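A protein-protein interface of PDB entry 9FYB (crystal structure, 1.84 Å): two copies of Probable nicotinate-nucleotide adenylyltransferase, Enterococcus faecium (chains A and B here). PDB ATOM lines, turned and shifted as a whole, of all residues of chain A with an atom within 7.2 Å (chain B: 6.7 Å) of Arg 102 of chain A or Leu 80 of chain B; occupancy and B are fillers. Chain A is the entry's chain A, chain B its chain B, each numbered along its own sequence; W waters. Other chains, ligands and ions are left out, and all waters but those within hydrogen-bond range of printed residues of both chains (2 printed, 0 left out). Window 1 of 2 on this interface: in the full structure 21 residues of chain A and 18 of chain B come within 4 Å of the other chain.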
ATOM      1  N   TYR A  63      -2.042 -20.224 -17.164  1.00  0.00           N
ATOM      2  CA  TYR A  63      -2.609 -18.934 -17.519  1.00  0.00           C
ATOM      3  C   TYR A  63      -3.987 -18.773 -16.867  1.00  0.00           C
ATOM      4  O   TYR A  63      -4.196 -17.865 -16.058  1.00  0.00           O
ATOM      5  CB  TYR A  63      -2.698 -18.787 -19.041  1.00  0.00           C
ATOM      6  CG  TYR A  63      -3.141 -17.417 -19.501  1.00  0.00           C
ATOM      7  CD1 TYR A  63      -2.208 -16.397 -19.702  1.00  0.00           C
ATOM      8  CD2 TYR A  63      -4.484 -17.143 -19.753  1.00  0.00           C
ATOM      9  CE1 TYR A  63      -2.603 -15.132 -20.126  1.00  0.00           C
ATOM     10  CE2 TYR A  63      -4.888 -15.881 -20.184  1.00  0.00           C
ATOM     11  CZ  TYR A  63      -3.942 -14.882 -20.367  1.00  0.00           C
ATOM     12  OH  TYR A  63      -4.340 -13.628 -20.785  1.00  0.00           O
ATOM     13  N   THR A  97       7.513 -20.722 -19.577  1.00  0.00           N
ATOM     14  CA  THR A  97       6.452 -19.745 -19.800  1.00  0.00           C
ATOM     15  C   THR A  97       5.523 -20.084 -20.973  1.00  0.00           C
ATOM     16  O   THR A  97       4.755 -19.216 -21.391  1.00  0.00           O
ATOM     17  CB  THR A  97       7.042 -18.340 -19.983  1.00  0.00           C
ATOM     18  OG1 THR A  97       7.978 -18.319 -21.069  1.00  0.00           O
ATOM     19  CG2 THR A  97       7.749 -17.897 -18.734  1.00  0.00           C
ATOM     20  N   ILE A  98       5.505 -21.332 -21.468  1.00  0.00           N
ATOM     21  CA  ILE A  98       4.701 -21.604 -22.670  1.00  0.00           C
ATOM     22  C   ILE A  98       3.212 -21.405 -22.394  1.00  0.00           C
ATOM     23  O   ILE A  98       2.465 -20.925 -23.261  1.00  0.00           O
ATOM     24  CB  ILE A  98       4.985 -23.015 -23.217  1.00  0.00           C
ATOM     25  CG1 ILE A  98       4.269 -23.230 -24.557  1.00  0.00           C
ATOM     26  CG2 ILE A  98       4.580 -24.085 -22.209  1.00  0.00           C
ATOM     27  CD1 ILE A  98       4.656 -24.545 -25.254  1.00  0.00           C
ATOM     28  N   GLU A  99       2.752 -21.743 -21.182  1.00  0.00           N
ATOM     29  CA  GLU A  99       1.319 -21.641 -20.916  1.00  0.00           C
ATOM     30  C   GLU A  99       0.890 -20.188 -20.765  1.00  0.00           C
ATOM     31  O   GLU A  99      -0.234 -19.840 -21.129  1.00  0.00           O
ATOM     32  CB  GLU A  99       0.947 -22.460 -19.675  1.00  0.00           C
ATOM     33  CG  GLU A  99       0.916 -23.970 -19.960  1.00  0.00           C
ATOM     34  CD  GLU A  99       0.267 -24.791 -18.850  1.00  0.00           C
ATOM     35  OE1 GLU A  99       0.056 -24.237 -17.749  1.00  0.00           O
ATOM     36  OE2 GLU A  99       0.026 -26.005 -19.055  1.00  0.00           O
ATOM     37  N   LEU A 100       1.778 -19.318 -20.284  1.00  0.00           N
ATOM     38  CA  LEU A 100       1.467 -17.887 -20.269  1.00  0.00           C
ATOM     39  C   LEU A 100       1.389 -17.309 -21.671  1.00  0.00           C
ATOM     40  O   LEU A 100       0.674 -16.327 -21.900  1.00  0.00           O
ATOM     41  CB  LEU A 100       2.534 -17.118 -19.511  1.00  0.00           C
ATOM     42  CG  LEU A 100       2.613 -17.327 -18.009  1.00  0.00           C
ATOM     43  CD1 LEU A 100       3.537 -16.293 -17.476  1.00  0.00           C
ATOM     44  CD2 LEU A 100       1.246 -17.246 -17.366  1.00  0.00           C
ATOM     45  N   ALA A 101       2.148 -17.871 -22.612  1.00  0.00           N
ATOM     46  CA  ALA A 101       2.236 -17.245 -23.922  1.00  0.00           C
ATOM     47  C   ALA A 101       1.025 -17.562 -24.771  1.00  0.00           C
ATOM     48  O   ALA A 101       0.568 -16.704 -25.534  1.00  0.00           O
ATOM     49  CB  ALA A 101       3.507 -17.681 -24.635  1.00  0.00           C
ATOM     50  N   ARG A 102       0.523 -18.785 -24.621  1.00  0.00           N
ATOM     51  CA  ARG A 102      -0.639 -19.220 -25.429  1.00  0.00           C
ATOM     52  C   ARG A 102      -1.811 -18.313 -25.071  1.00  0.00           C
ATOM     53  O   ARG A 102      -2.633 -18.041 -25.955  1.00  0.00           O
ATOM     54  CB  ARG A 102      -0.908 -20.710 -25.203  1.00  0.00           C
ATOM     55  CG  ARG A 102       0.295 -21.594 -25.504  1.00  0.00           C
ATOM     56  CD  ARG A 102      -0.062 -22.965 -26.038  1.00  0.00           C
ATOM     57  NE  ARG A 102      -0.077 -23.982 -24.998  1.00  0.00           N
ATOM     58  CZ  ARG A 102      -1.180 -24.521 -24.494  1.00  0.00           C
ATOM     59  NH1 ARG A 102      -2.351 -23.945 -24.703  1.00  0.00           N
ATOM     60  NH2 ARG A 102      -1.112 -25.633 -23.786  1.00  0.00           N
ATOM     61  N   GLY A 103      -1.864 -17.858 -23.823  1.00  0.00           N
ATOM     62  CA  GLY A 103      -2.907 -16.904 -23.415  1.00  0.00           C
ATOM     63  C   GLY A 103      -4.287 -17.520 -23.402  1.00  0.00           C
ATOM     64  O   GLY A 103      -5.205 -16.907 -23.975  1.00  0.00           O
ATOM     65  N   GLY A 104      -4.446 -18.674 -22.759  1.00  0.00           N
ATOM     66  CA  GLY A 104      -5.803 -19.238 -22.641  1.00  0.00           C
ATOM     67  C   GLY A 104      -5.828 -20.485 -21.782  1.00  0.00           C
ATOM     68  O   GLY A 104      -4.748 -20.912 -21.351  1.00  0.00           O
ATOM     69  N   LYS A 105      -7.016 -21.034 -21.528  1.00  0.00           N
ATOM     70  CA  LYS A 105      -7.101 -22.318 -20.792  1.00  0.00           C
ATOM     71  C   LYS A 105      -6.168 -23.297 -21.494  1.00  0.00           C
ATOM     72  O   LYS A 105      -6.367 -23.532 -22.698  1.00  0.00           O
ATOM     73  CB  LYS A 105      -8.528 -22.860 -20.819  1.00  0.00           C
ATOM     74  CG  LYS A 105      -9.173 -23.051 -19.456  1.00  0.00           C
ATOM     75  CD  LYS A 105     -10.450 -23.846 -19.533  1.00  0.00           C
ATOM     76  CE  LYS A 105     -10.393 -25.116 -18.716  1.00  0.00           C
ATOM     77  NZ  LYS A 105      -9.001 -25.506 -18.393  1.00  0.00           N
ATOM     78  N   SER A 106      -5.201 -23.851 -20.767  1.00  0.00           N
ATOM     79  CA  SER A 106      -4.230 -24.709 -21.441  1.00  0.00           C
ATOM     80  C   SER A 106      -4.278 -26.096 -20.808  1.00  0.00           C
ATOM     81  O   SER A 106      -3.899 -26.266 -19.643  1.00  0.00           O
ATOM     82  CB  SER A 106      -2.823 -24.107 -21.350  1.00  0.00           C
ATOM     83  OG  SER A 106      -2.822 -22.700 -21.590  1.00  0.00           O
ATOM     84  N   TYR A 107      -4.736 -27.088 -21.568  1.00  0.00           N
ATOM     85  CA  TYR A 107      -4.814 -28.451 -21.049  1.00  0.00           C
ATOM     86  C   TYR A 107      -3.438 -29.108 -21.062  1.00  0.00           C
ATOM     87  O   TYR A 107      -2.715 -29.034 -22.064  1.00  0.00           O
ATOM     88  CB  TYR A 107      -5.815 -29.296 -21.844  1.00  0.00           C
ATOM     89  CG  TYR A 107      -7.258 -28.868 -21.673  1.00  0.00           C
ATOM     90  CD1 TYR A 107      -7.616 -27.524 -21.657  1.00  0.00           C
ATOM     91  CD2 TYR A 107      -8.259 -29.810 -21.454  1.00  0.00           C
ATOM     92  CE1 TYR A 107      -8.924 -27.133 -21.483  1.00  0.00           C
ATOM     93  CE2 TYR A 107      -9.576 -29.424 -21.268  1.00  0.00           C
ATOM     94  CZ  TYR A 107      -9.903 -28.079 -21.283  1.00  0.00           C
ATOM     95  OH  TYR A 107     -11.206 -27.666 -21.104  1.00  0.00           O
ATOM     96  N   THR A 108      -3.080 -29.752 -19.942  1.00  0.00           N
ATOM     97  CA  THR A 108      -1.747 -30.333 -19.792  1.00  0.00           C
ATOM     98  C   THR A 108      -1.353 -31.180 -20.995  1.00  0.00           C
ATOM     99  O   THR A 108      -0.184 -31.175 -21.396  1.00  0.00           O
ATOM    100  CB  THR A 108      -1.680 -31.166 -18.512  1.00  0.00           C
ATOM    101  OG1 THR A 108      -1.926 -30.316 -17.385  1.00  0.00           O
ATOM    102  CG2 THR A 108      -0.297 -31.794 -18.353  1.00  0.00           C
ATOM    103  N   TYR A 109      -2.319 -31.850 -21.627  1.00  0.00           N
ATOM    104  CA  TYR A 109      -2.021 -32.659 -22.809  1.00  0.00           C
ATOM    105  C   TYR A 109      -1.427 -31.813 -23.925  1.00  0.00           C
ATOM    106  O   TYR A 109      -0.377 -32.146 -24.487  1.00  0.00           O
ATOM    107  CB  TYR A 109      -3.279 -33.365 -23.313  1.00  0.00           C
ATOM    108  CG  TYR A 109      -3.034 -33.993 -24.656  1.00  0.00           C
ATOM    109  CD1 TYR A 109      -2.277 -35.149 -24.766  1.00  0.00           C
ATOM    110  CD2 TYR A 109      -3.513 -33.403 -25.823  1.00  0.00           C
ATOM    111  CE1 TYR A 109      -2.027 -35.716 -25.987  1.00  0.00           C
ATOM    112  CE2 TYR A 109      -3.270 -33.967 -27.046  1.00  0.00           C
ATOM    113  CZ  TYR A 109      -2.522 -35.123 -27.122  1.00  0.00           C
ATOM    114  OH  TYR A 109      -2.270 -35.693 -28.344  1.00  0.00           O
ATOM    115  N   ASP A 110      -2.106 -30.717 -24.277  1.00  0.00           N
ATOM    116  CA  ASP A 110      -1.606 -29.842 -25.329  1.00  0.00           C
ATOM    117  C   ASP A 110      -0.269 -29.244 -24.943  1.00  0.00           C
ATOM    118  O   ASP A 110       0.645 -29.154 -25.774  1.00  0.00           O
ATOM    119  CB  ASP A 110      -2.613 -28.732 -25.613  1.00  0.00           C
ATOM    120  CG  ASP A 110      -3.959 -29.269 -26.009  1.00  0.00           C
ATOM    121  OD1 ASP A 110      -4.026 -29.925 -27.068  1.00  0.00           O
ATOM    122  OD2 ASP A 110      -4.934 -29.049 -25.257  1.00  0.00           O
ATOM    123  N   THR A 111      -0.137 -28.827 -23.684  1.00  0.00           N
ATOM    124  CA  THR A 111       1.135 -28.283 -23.233  1.00  0.00           C
ATOM    125  C   THR A 111       2.258 -29.291 -23.429  1.00  0.00           C
ATOM    126  O   THR A 111       3.286 -28.979 -24.043  1.00  0.00           O
ATOM    127  CB  THR A 111       1.039 -27.870 -21.778  1.00  0.00           C
ATOM    128  OG1 THR A 111       0.014 -26.880 -21.645  1.00  0.00           O
ATOM    129  CG2 THR A 111       2.375 -27.310 -21.314  1.00  0.00           C
ATOM    130  N   MET A 112       2.062 -30.523 -22.959  1.00  0.00           N
ATOM    131  CA  MET A 112       3.157 -31.468 -23.019  1.00  0.00           C
ATOM    132  C   MET A 112       3.340 -31.964 -24.442  1.00  0.00           C
ATOM    133  O   MET A 112       4.440 -32.376 -24.809  1.00  0.00           O
ATOM    134  CB  MET A 112       2.885 -32.636 -22.070  1.00  0.00           C
ATOM    135  CG  MET A 112       3.213 -32.320 -20.602  1.00  0.00           C
ATOM    136  SD  MET A 112       4.470 -31.076 -20.209  1.00  0.00           S
ATOM    137  CE  MET A 112       5.955 -31.782 -20.965  1.00  0.00           C
ATOM    138  N   GLU A 114       3.215 -29.908 -27.032  1.00  0.00           N
ATOM    139  CA  GLU A 114       4.100 -28.935 -27.671  1.00  0.00           C
ATOM    140  C   GLU A 114       5.530 -29.065 -27.165  1.00  0.00           C
ATOM    141  O   GLU A 114       6.482 -28.992 -27.958  1.00  0.00           O
ATOM    142  CB  GLU A 114       3.560 -27.519 -27.464  1.00  0.00           C
ATOM    143  CG  GLU A 114       4.328 -26.474 -28.246  1.00  0.00           C
ATOM    144  CD  GLU A 114       3.467 -25.297 -28.660  1.00  0.00           C
ATOM    145  OE1 GLU A 114       3.995 -24.362 -29.311  1.00  0.00           O
ATOM    146  OE2 GLU A 114       2.264 -25.310 -28.327  1.00  0.00           O
ATOM    147  N   PHE B  34       5.805 -11.482 -37.746  1.00  0.00           N
ATOM    148  CA  PHE B  34       4.889 -12.427 -38.393  1.00  0.00           C
ATOM    149  C   PHE B  34       3.455 -11.890 -38.374  1.00  0.00           C
ATOM    150  O   PHE B  34       2.545 -12.438 -37.756  1.00  0.00           O
ATOM    151  CB  PHE B  34       4.978 -13.802 -37.730  1.00  0.00           C
ATOM    152  CG  PHE B  34       6.374 -14.325 -37.636  1.00  0.00           C
ATOM    153  CD1 PHE B  34       6.948 -15.015 -38.701  1.00  0.00           C
ATOM    154  CD2 PHE B  34       7.119 -14.106 -36.488  1.00  0.00           C
ATOM    155  CE1 PHE B  34       8.245 -15.482 -38.621  1.00  0.00           C
ATOM    156  CE2 PHE B  34       8.421 -14.583 -36.390  1.00  0.00           C
ATOM    157  CZ  PHE B  34       8.984 -15.277 -37.469  1.00  0.00           C
ATOM    158  N   PRO B  61       8.027 -15.102 -32.525  1.00  0.00           N
ATOM    159  CA  PRO B  61       7.323 -13.827 -32.724  1.00  0.00           C
ATOM    160  C   PRO B  61       7.606 -12.868 -31.581  1.00  0.00           C
ATOM    161  O   PRO B  61       7.521 -13.243 -30.407  1.00  0.00           O
ATOM    162  CB  PRO B  61       5.846 -14.232 -32.765  1.00  0.00           C
ATOM    163  CG  PRO B  61       5.779 -15.523 -31.991  1.00  0.00           C
ATOM    164  CD  PRO B  61       7.106 -16.214 -32.256  1.00  0.00           C
ATOM    165  N   ASP B  75      -3.344  -8.412 -32.237  1.00  0.00           N
ATOM    166  CA  ASP B  75      -3.143  -9.164 -30.980  1.00  0.00           C
ATOM    167  C   ASP B  75      -2.070 -10.236 -31.138  1.00  0.00           C
ATOM    168  O   ASP B  75      -2.126 -10.998 -32.111  1.00  0.00           O
ATOM    169  CB  ASP B  75      -4.439  -9.821 -30.510  1.00  0.00           C
ATOM    170  CG  ASP B  75      -4.585  -9.832 -29.001  1.00  0.00           C
ATOM    171  OD1 ASP B  75      -3.822 -10.567 -28.346  1.00  0.00           O
ATOM    172  OD2 ASP B  75      -5.449  -9.096 -28.495  1.00  0.00           O
ATOM    173  N   ALA B  76      -1.146 -10.295 -30.188  1.00  0.00           N
ATOM    174  CA  ALA B  76      -0.164 -11.370 -30.175  1.00  0.00           C
ATOM    175  C   ALA B  76      -0.834 -12.737 -30.273  1.00  0.00           C
ATOM    176  O   ALA B  76      -0.354 -13.624 -30.987  1.00  0.00           O
ATOM    177  CB  ALA B  76       0.693 -11.276 -28.917  1.00  0.00           C
ATOM    178  N   LYS B  77      -1.957 -12.930 -29.588  1.00  0.00           N
ATOM    179  CA  LYS B  77      -2.565 -14.255 -29.642  1.00  0.00           C
ATOM    180  C   LYS B  77      -3.014 -14.593 -31.058  1.00  0.00           C
ATOM    181  O   LYS B  77      -2.964 -15.764 -31.470  1.00  0.00           O
ATOM    182  CB  LYS B  77      -3.725 -14.366 -28.653  1.00  0.00           C
ATOM    183  CG  LYS B  77      -4.710 -15.444 -29.014  1.00  0.00           C
ATOM    184  CD  LYS B  77      -4.109 -16.830 -28.721  1.00  0.00           C
ATOM    185  CE  LYS B  77      -5.154 -17.851 -28.286  1.00  0.00           C
ATOM    186  NZ  LYS B  77      -4.482 -19.144 -27.947  1.00  0.00           N
ATOM    187  N   HIS B  78      -3.408 -13.584 -31.839  1.00  0.00           N
ATOM    188  CA  HIS B  78      -3.738 -13.857 -33.233  1.00  0.00           C
ATOM    189  C   HIS B  78      -2.487 -14.271 -33.999  1.00  0.00           C
ATOM    190  O   HIS B  78      -2.502 -15.255 -34.748  1.00  0.00           O
ATOM    191  CB  HIS B  78      -4.397 -12.632 -33.877  1.00  0.00           C
ATOM    192  CG  HIS B  78      -5.848 -12.489 -33.546  1.00  0.00           C
ATOM    193  ND1 HIS B  78      -6.725 -13.555 -33.555  1.00  0.00           N
ATOM    194  CD2 HIS B  78      -6.573 -11.406 -33.173  1.00  0.00           C
ATOM    195  CE1 HIS B  78      -7.932 -13.131 -33.227  1.00  0.00           C
ATOM    196  NE2 HIS B  78      -7.866 -11.831 -32.986  1.00  0.00           N
ATOM    197  N   ARG B  79      -1.389 -13.532 -33.826  1.00  0.00           N
ATOM    198  CA  ARG B  79      -0.175 -13.879 -34.556  1.00  0.00           C
ATOM    199  C   ARG B  79       0.338 -15.260 -34.149  1.00  0.00           C
ATOM    200  O   ARG B  79       0.816 -16.032 -34.995  1.00  0.00           O
ATOM    201  CB  ARG B  79       0.875 -12.797 -34.337  1.00  0.00           C
ATOM    202  CG  ARG B  79       0.392 -11.429 -34.807  1.00  0.00           C
ATOM    203  CD  ARG B  79       1.469 -10.372 -34.734  1.00  0.00           C
ATOM    204  NE  ARG B  79       1.641  -9.887 -33.370  1.00  0.00           N
ATOM    205  CZ  ARG B  79       2.771  -9.985 -32.686  1.00  0.00           C
ATOM    206  NH1 ARG B  79       3.848 -10.541 -33.210  1.00  0.00           N
ATOM    207  NH2 ARG B  79       2.821  -9.517 -31.442  1.00  0.00           N
ATOM    208  N   LEU B  80       0.210 -15.604 -32.858  1.00  0.00           N
ATOM    209  CA  LEU B  80       0.636 -16.915 -32.374  1.00  0.00           C
ATOM    210  C   LEU B  80      -0.205 -18.028 -32.975  1.00  0.00           C
ATOM    211  O   LEU B  80       0.326 -19.070 -33.375  1.00  0.00           O
ATOM    212  CB  LEU B  80       0.570 -16.965 -30.839  1.00  0.00           C
ATOM    213  CG  LEU B  80       0.802 -18.343 -30.205  1.00  0.00           C
ATOM    214  CD1 LEU B  80       2.229 -18.798 -30.501  1.00  0.00           C
ATOM    215  CD2 LEU B  80       0.554 -18.290 -28.669  1.00  0.00           C
ATOM    216  N   ASN B  81      -1.530 -17.843 -33.030  1.00  0.00           N
ATOM    217  CA  ASN B  81      -2.383 -18.866 -33.629  1.00  0.00           C
ATOM    218  C   ASN B  81      -2.032 -19.088 -35.103  1.00  0.00           C
ATOM    219  O   ASN B  81      -1.914 -20.224 -35.566  1.00  0.00           O
ATOM    220  CB  ASN B  81      -3.860 -18.483 -33.486  1.00  0.00           C
ATOM    221  CG  ASN B  81      -4.412 -18.742 -32.080  1.00  0.00           C
ATOM    222  OD1 ASN B  81      -3.838 -19.507 -31.305  1.00  0.00           O
ATOM    223  ND2 ASN B  81      -5.542 -18.126 -31.767  1.00  0.00           N
ATOM    224  N   MET B  82      -1.855 -18.010 -35.854  1.00  0.00           N
ATOM    225  CA  MET B  82      -1.516 -18.141 -37.268  1.00  0.00           C
ATOM    226  C   MET B  82      -0.213 -18.925 -37.431  1.00  0.00           C
ATOM    227  O   MET B  82      -0.117 -19.860 -38.245  1.00  0.00           O
ATOM    228  CB  MET B  82      -1.403 -16.730 -37.835  1.00  0.00           C
ATOM    229  CG  MET B  82      -2.771 -16.043 -37.897  1.00  0.00           C
ATOM    230  SD  MET B  82      -2.896 -14.661 -39.031  1.00  0.00           S
ATOM    231  CE  MET B  82      -2.087 -13.450 -38.014  1.00  0.00           C
ATOM    232  N   LEU B  83       0.784 -18.589 -36.610  1.00  0.00           N
ATOM    233  CA  LEU B  83       2.075 -19.264 -36.695  1.00  0.00           C
ATOM    234  C   LEU B  83       1.939 -20.745 -36.422  1.00  0.00           C
ATOM    235  O   LEU B  83       2.622 -21.570 -37.048  1.00  0.00           O
ATOM    236  CB  LEU B  83       3.062 -18.666 -35.702  1.00  0.00           C
ATOM    237  CG  LEU B  83       3.711 -17.366 -36.136  1.00  0.00           C
ATOM    238  CD1 LEU B  83       4.109 -16.563 -34.910  1.00  0.00           C
ATOM    239  CD2 LEU B  83       4.901 -17.705 -37.046  1.00  0.00           C
ATOM    240  N   GLU B  84       1.096 -21.102 -35.460  1.00  0.00           N
ATOM    241  CA  GLU B  84       1.062 -22.498 -35.068  1.00  0.00           C
ATOM    242  C   GLU B  84       0.411 -23.315 -36.159  1.00  0.00           C
ATOM    243  O   GLU B  84       0.823 -24.449 -36.433  1.00  0.00           O
ATOM    244  CB  GLU B  84       0.323 -22.683 -33.743  1.00  0.00           C
ATOM    245  CG  GLU B  84       1.089 -22.053 -32.599  1.00  0.00           C
ATOM    246  CD  GLU B  84       1.886 -23.061 -31.802  1.00  0.00           C
ATOM    247  OE1 GLU B  84       2.381 -22.687 -30.726  1.00  0.00           O
ATOM    248  OE2 GLU B  84       2.142 -24.181 -32.321  1.00  0.00           O
ATOM    249  N   LEU B  85      -0.615 -22.742 -36.794  1.00  0.00           N
ATOM    250  CA  LEU B  85      -1.206 -23.352 -37.972  1.00  0.00           C
ATOM    251  C   LEU B  85      -0.221 -23.416 -39.130  1.00  0.00           C
ATOM    252  O   LEU B  85      -0.304 -24.331 -39.949  1.00  0.00           O
ATOM    253  CB  LEU B  85      -2.447 -22.578 -38.411  1.00  0.00           C
ATOM    254  CG  LEU B  85      -3.643 -22.561 -37.454  1.00  0.00           C
ATOM    255  CD1 LEU B  85      -4.522 -21.325 -37.718  1.00  0.00           C
ATOM    256  CD2 LEU B  85      -4.419 -23.868 -37.586  1.00  0.00           C
ATOM    257  N   ILE B  95       7.581 -23.263 -32.831  1.00  0.00           N
ATOM    258  CA  ILE B  95       7.340 -21.891 -32.409  1.00  0.00           C
ATOM    259  C   ILE B  95       7.996 -21.692 -31.050  1.00  0.00           C
ATOM    260  O   ILE B  95       7.871 -22.547 -30.160  1.00  0.00           O
ATOM    261  CB  ILE B  95       5.833 -21.588 -32.343  1.00  0.00           C
ATOM    262  CG1 ILE B  95       5.136 -21.967 -33.650  1.00  0.00           C
ATOM    263  CG2 ILE B  95       5.596 -20.141 -31.984  1.00  0.00           C
ATOM    264  CD1 ILE B  95       5.680 -21.230 -34.888  1.00  0.00           C
ATOM    265  N   GLU B  96       8.702 -20.575 -30.894  1.00  0.00           N
ATOM    266  CA  GLU B  96       9.310 -20.175 -29.627  1.00  0.00           C
ATOM    267  C   GLU B  96       8.540 -18.979 -29.075  1.00  0.00           C
ATOM    268  O   GLU B  96       8.589 -17.886 -29.644  1.00  0.00           O
ATOM    269  CB  GLU B  96      10.789 -19.829 -29.822  1.00  0.00           C
ATOM    270  CG  GLU B  96      11.421 -19.157 -28.626  1.00  0.00           C
ATOM    271  CD  GLU B  96      11.276 -19.994 -27.351  1.00  0.00           C
ATOM    272  OE1 GLU B  96      11.862 -21.099 -27.290  1.00  0.00           O
ATOM    273  OE2 GLU B  96      10.560 -19.536 -26.431  1.00  0.00           O
ATOM    274  N   THR B  97       7.838 -19.176 -27.957  1.00  0.00           N
ATOM    275  CA  THR B  97       6.875 -18.196 -27.468  1.00  0.00           C
ATOM    276  C   THR B  97       7.388 -17.306 -26.335  1.00  0.00           C
ATOM    277  O   THR B  97       6.601 -16.528 -25.786  1.00  0.00           O
ATOM    278  CB  THR B  97       5.605 -18.915 -27.012  1.00  0.00           C
ATOM    279  OG1 THR B  97       5.949 -19.864 -25.998  1.00  0.00           O
ATOM    280  CG2 THR B  97       4.979 -19.645 -28.176  1.00  0.00           C
ATOM    281  N   LEU B 100       6.465 -13.639 -26.270  1.00  0.00           N
ATOM    282  CA  LEU B 100       5.050 -13.351 -26.079  1.00  0.00           C
ATOM    283  C   LEU B 100       4.642 -13.527 -24.621  1.00  0.00           C
ATOM    284  O   LEU B 100       3.763 -12.810 -24.133  1.00  0.00           O
ATOM    285  CB  LEU B 100       4.188 -14.252 -26.971  1.00  0.00           C
ATOM    286  CG  LEU B 100       4.241 -14.057 -28.493  1.00  0.00           C
ATOM    287  CD1 LEU B 100       3.148 -14.839 -29.206  1.00  0.00           C
ATOM    288  CD2 LEU B 100       4.199 -12.589 -28.898  1.00  0.00           C
ATOM    289  N   ALA B 101       5.255 -14.482 -23.919  1.00  0.00           N
ATOM    290  CA  ALA B 101       4.997 -14.630 -22.491  1.00  0.00           C
ATOM    291  C   ALA B 101       5.634 -13.500 -21.692  1.00  0.00           C
ATOM    292  O   ALA B 101       5.002 -12.943 -20.793  1.00  0.00           O
ATOM    293  CB  ALA B 101       5.514 -15.981 -22.001  1.00  0.00           C
HETATM  294  O   HOH W   1       6.004 -25.130 -31.559  1.00  0.00           O
HETATM  295  O   HOH W   2       6.195 -23.427 -28.247  1.00  0.00           O
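The backbone carbonyl oxygen of Arg 102 of chain A lies within hydrogen-bond range of the side-chain amino group of Lys 77 of chain B, at 2.9 Å.
The side-chain carboxylate of Glu 114 of chain A lies close to the side-chain carboxylate of Glu 84 of chain B (2.7 Å).
NH2 of Arg 102 of chain A lies within hydrogen-bond range of OG1 of Thr 111 of chain A (2.7 Å).
The backbone NH (N) of Lys 77 of chain B lies close to the side-chain carboxylate (OD1) of Asp 75 of chain B.
NZ of Lys 77 of chain B lies within hydrogen-bond range of OD1 of Asn 81 of chain B, at 3.4 Å.
The guanidinium group of Arg 102 of chain A is in hydrogen-bond range of the side-chain hydroxyl of Ser 106 of chain A (3.4 Å).
Among the printed residues, pairs that only touch across the chains: Thr 97 of chain A with Ala 101 of chain B (3.4 Å), Ile 98 of chain A with Thr 97 of chain B (3.96 Å), Ala 101 of chain A with Leu 80 of chain B (3.5 Å), Ala 101 of chain A with Thr 97 of chain B (3.4 Å), Ala 101 of chain A with Ala 101 of chain B (3.7 Å) and Arg 102 of chain A with Leu 80 of chain B (3.6 Å).
Arg 102 of chain A touches just these residues of chain B: Lys 77 and Leu 80.
Of the printed residues of chain B, Glu 114 of chain A touches Glu 84.
Leu 80 of chain B touches two residues of chain A.
Of the printed residues of chain A, Glu 84 of chain B touches Glu 114.
The nearest residue of chain A that does not touch Leu 80 of chain B is Gly 103 of chain A (5.4 Å).
The nearest printed residue of chain A that does not touch Thr 97 of chain B is Thr 97 of chain A (4.8 Å).
Printed residues of chain B that touch a printed residue of chain A: Lys 77, Leu 80, Glu 84, Thr 97 and Ala 101.
Hydrophobic or aromatic side chains of chain B that line the printed part of chain A: Leu 80 and Ala 101.
Along chain B the printed residues that touch a printed residue of chain A span positions 77 to 101.
Of the 18 printed residues of chain A, 5 touch a printed residue of chain B.
Printed residues of chain A that touch a printed residue of chain B: Thr 97, Ile 98, Ala 101, Arg 102 and Glu 114.
Thr 97 of chain A touches Ala 101 of chain B, and with the chains exchanged Ala 101 of chain A touches Thr 97 of chain B.
Ala 101 of chain A touches its own counterpart, Ala 101 of chain B.
3 positions are printed for both chains.
Of the 8 pairs that touch across the chains among the printed residues, 3 have their exchanged pair printed and touching as well.
Water W2 lies within hydrogen-bond range of OE1 of Glu 114 of chain A (2.6 Å) and O of Ile 95 of chain B (2.7 Å).
Water W1 lies within hydrogen-bond range of the backbone NH of Ile 95 of chain B (2.8 Å) and the side-chain carboxylate of Glu 114 of chain A (3.1 Å).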
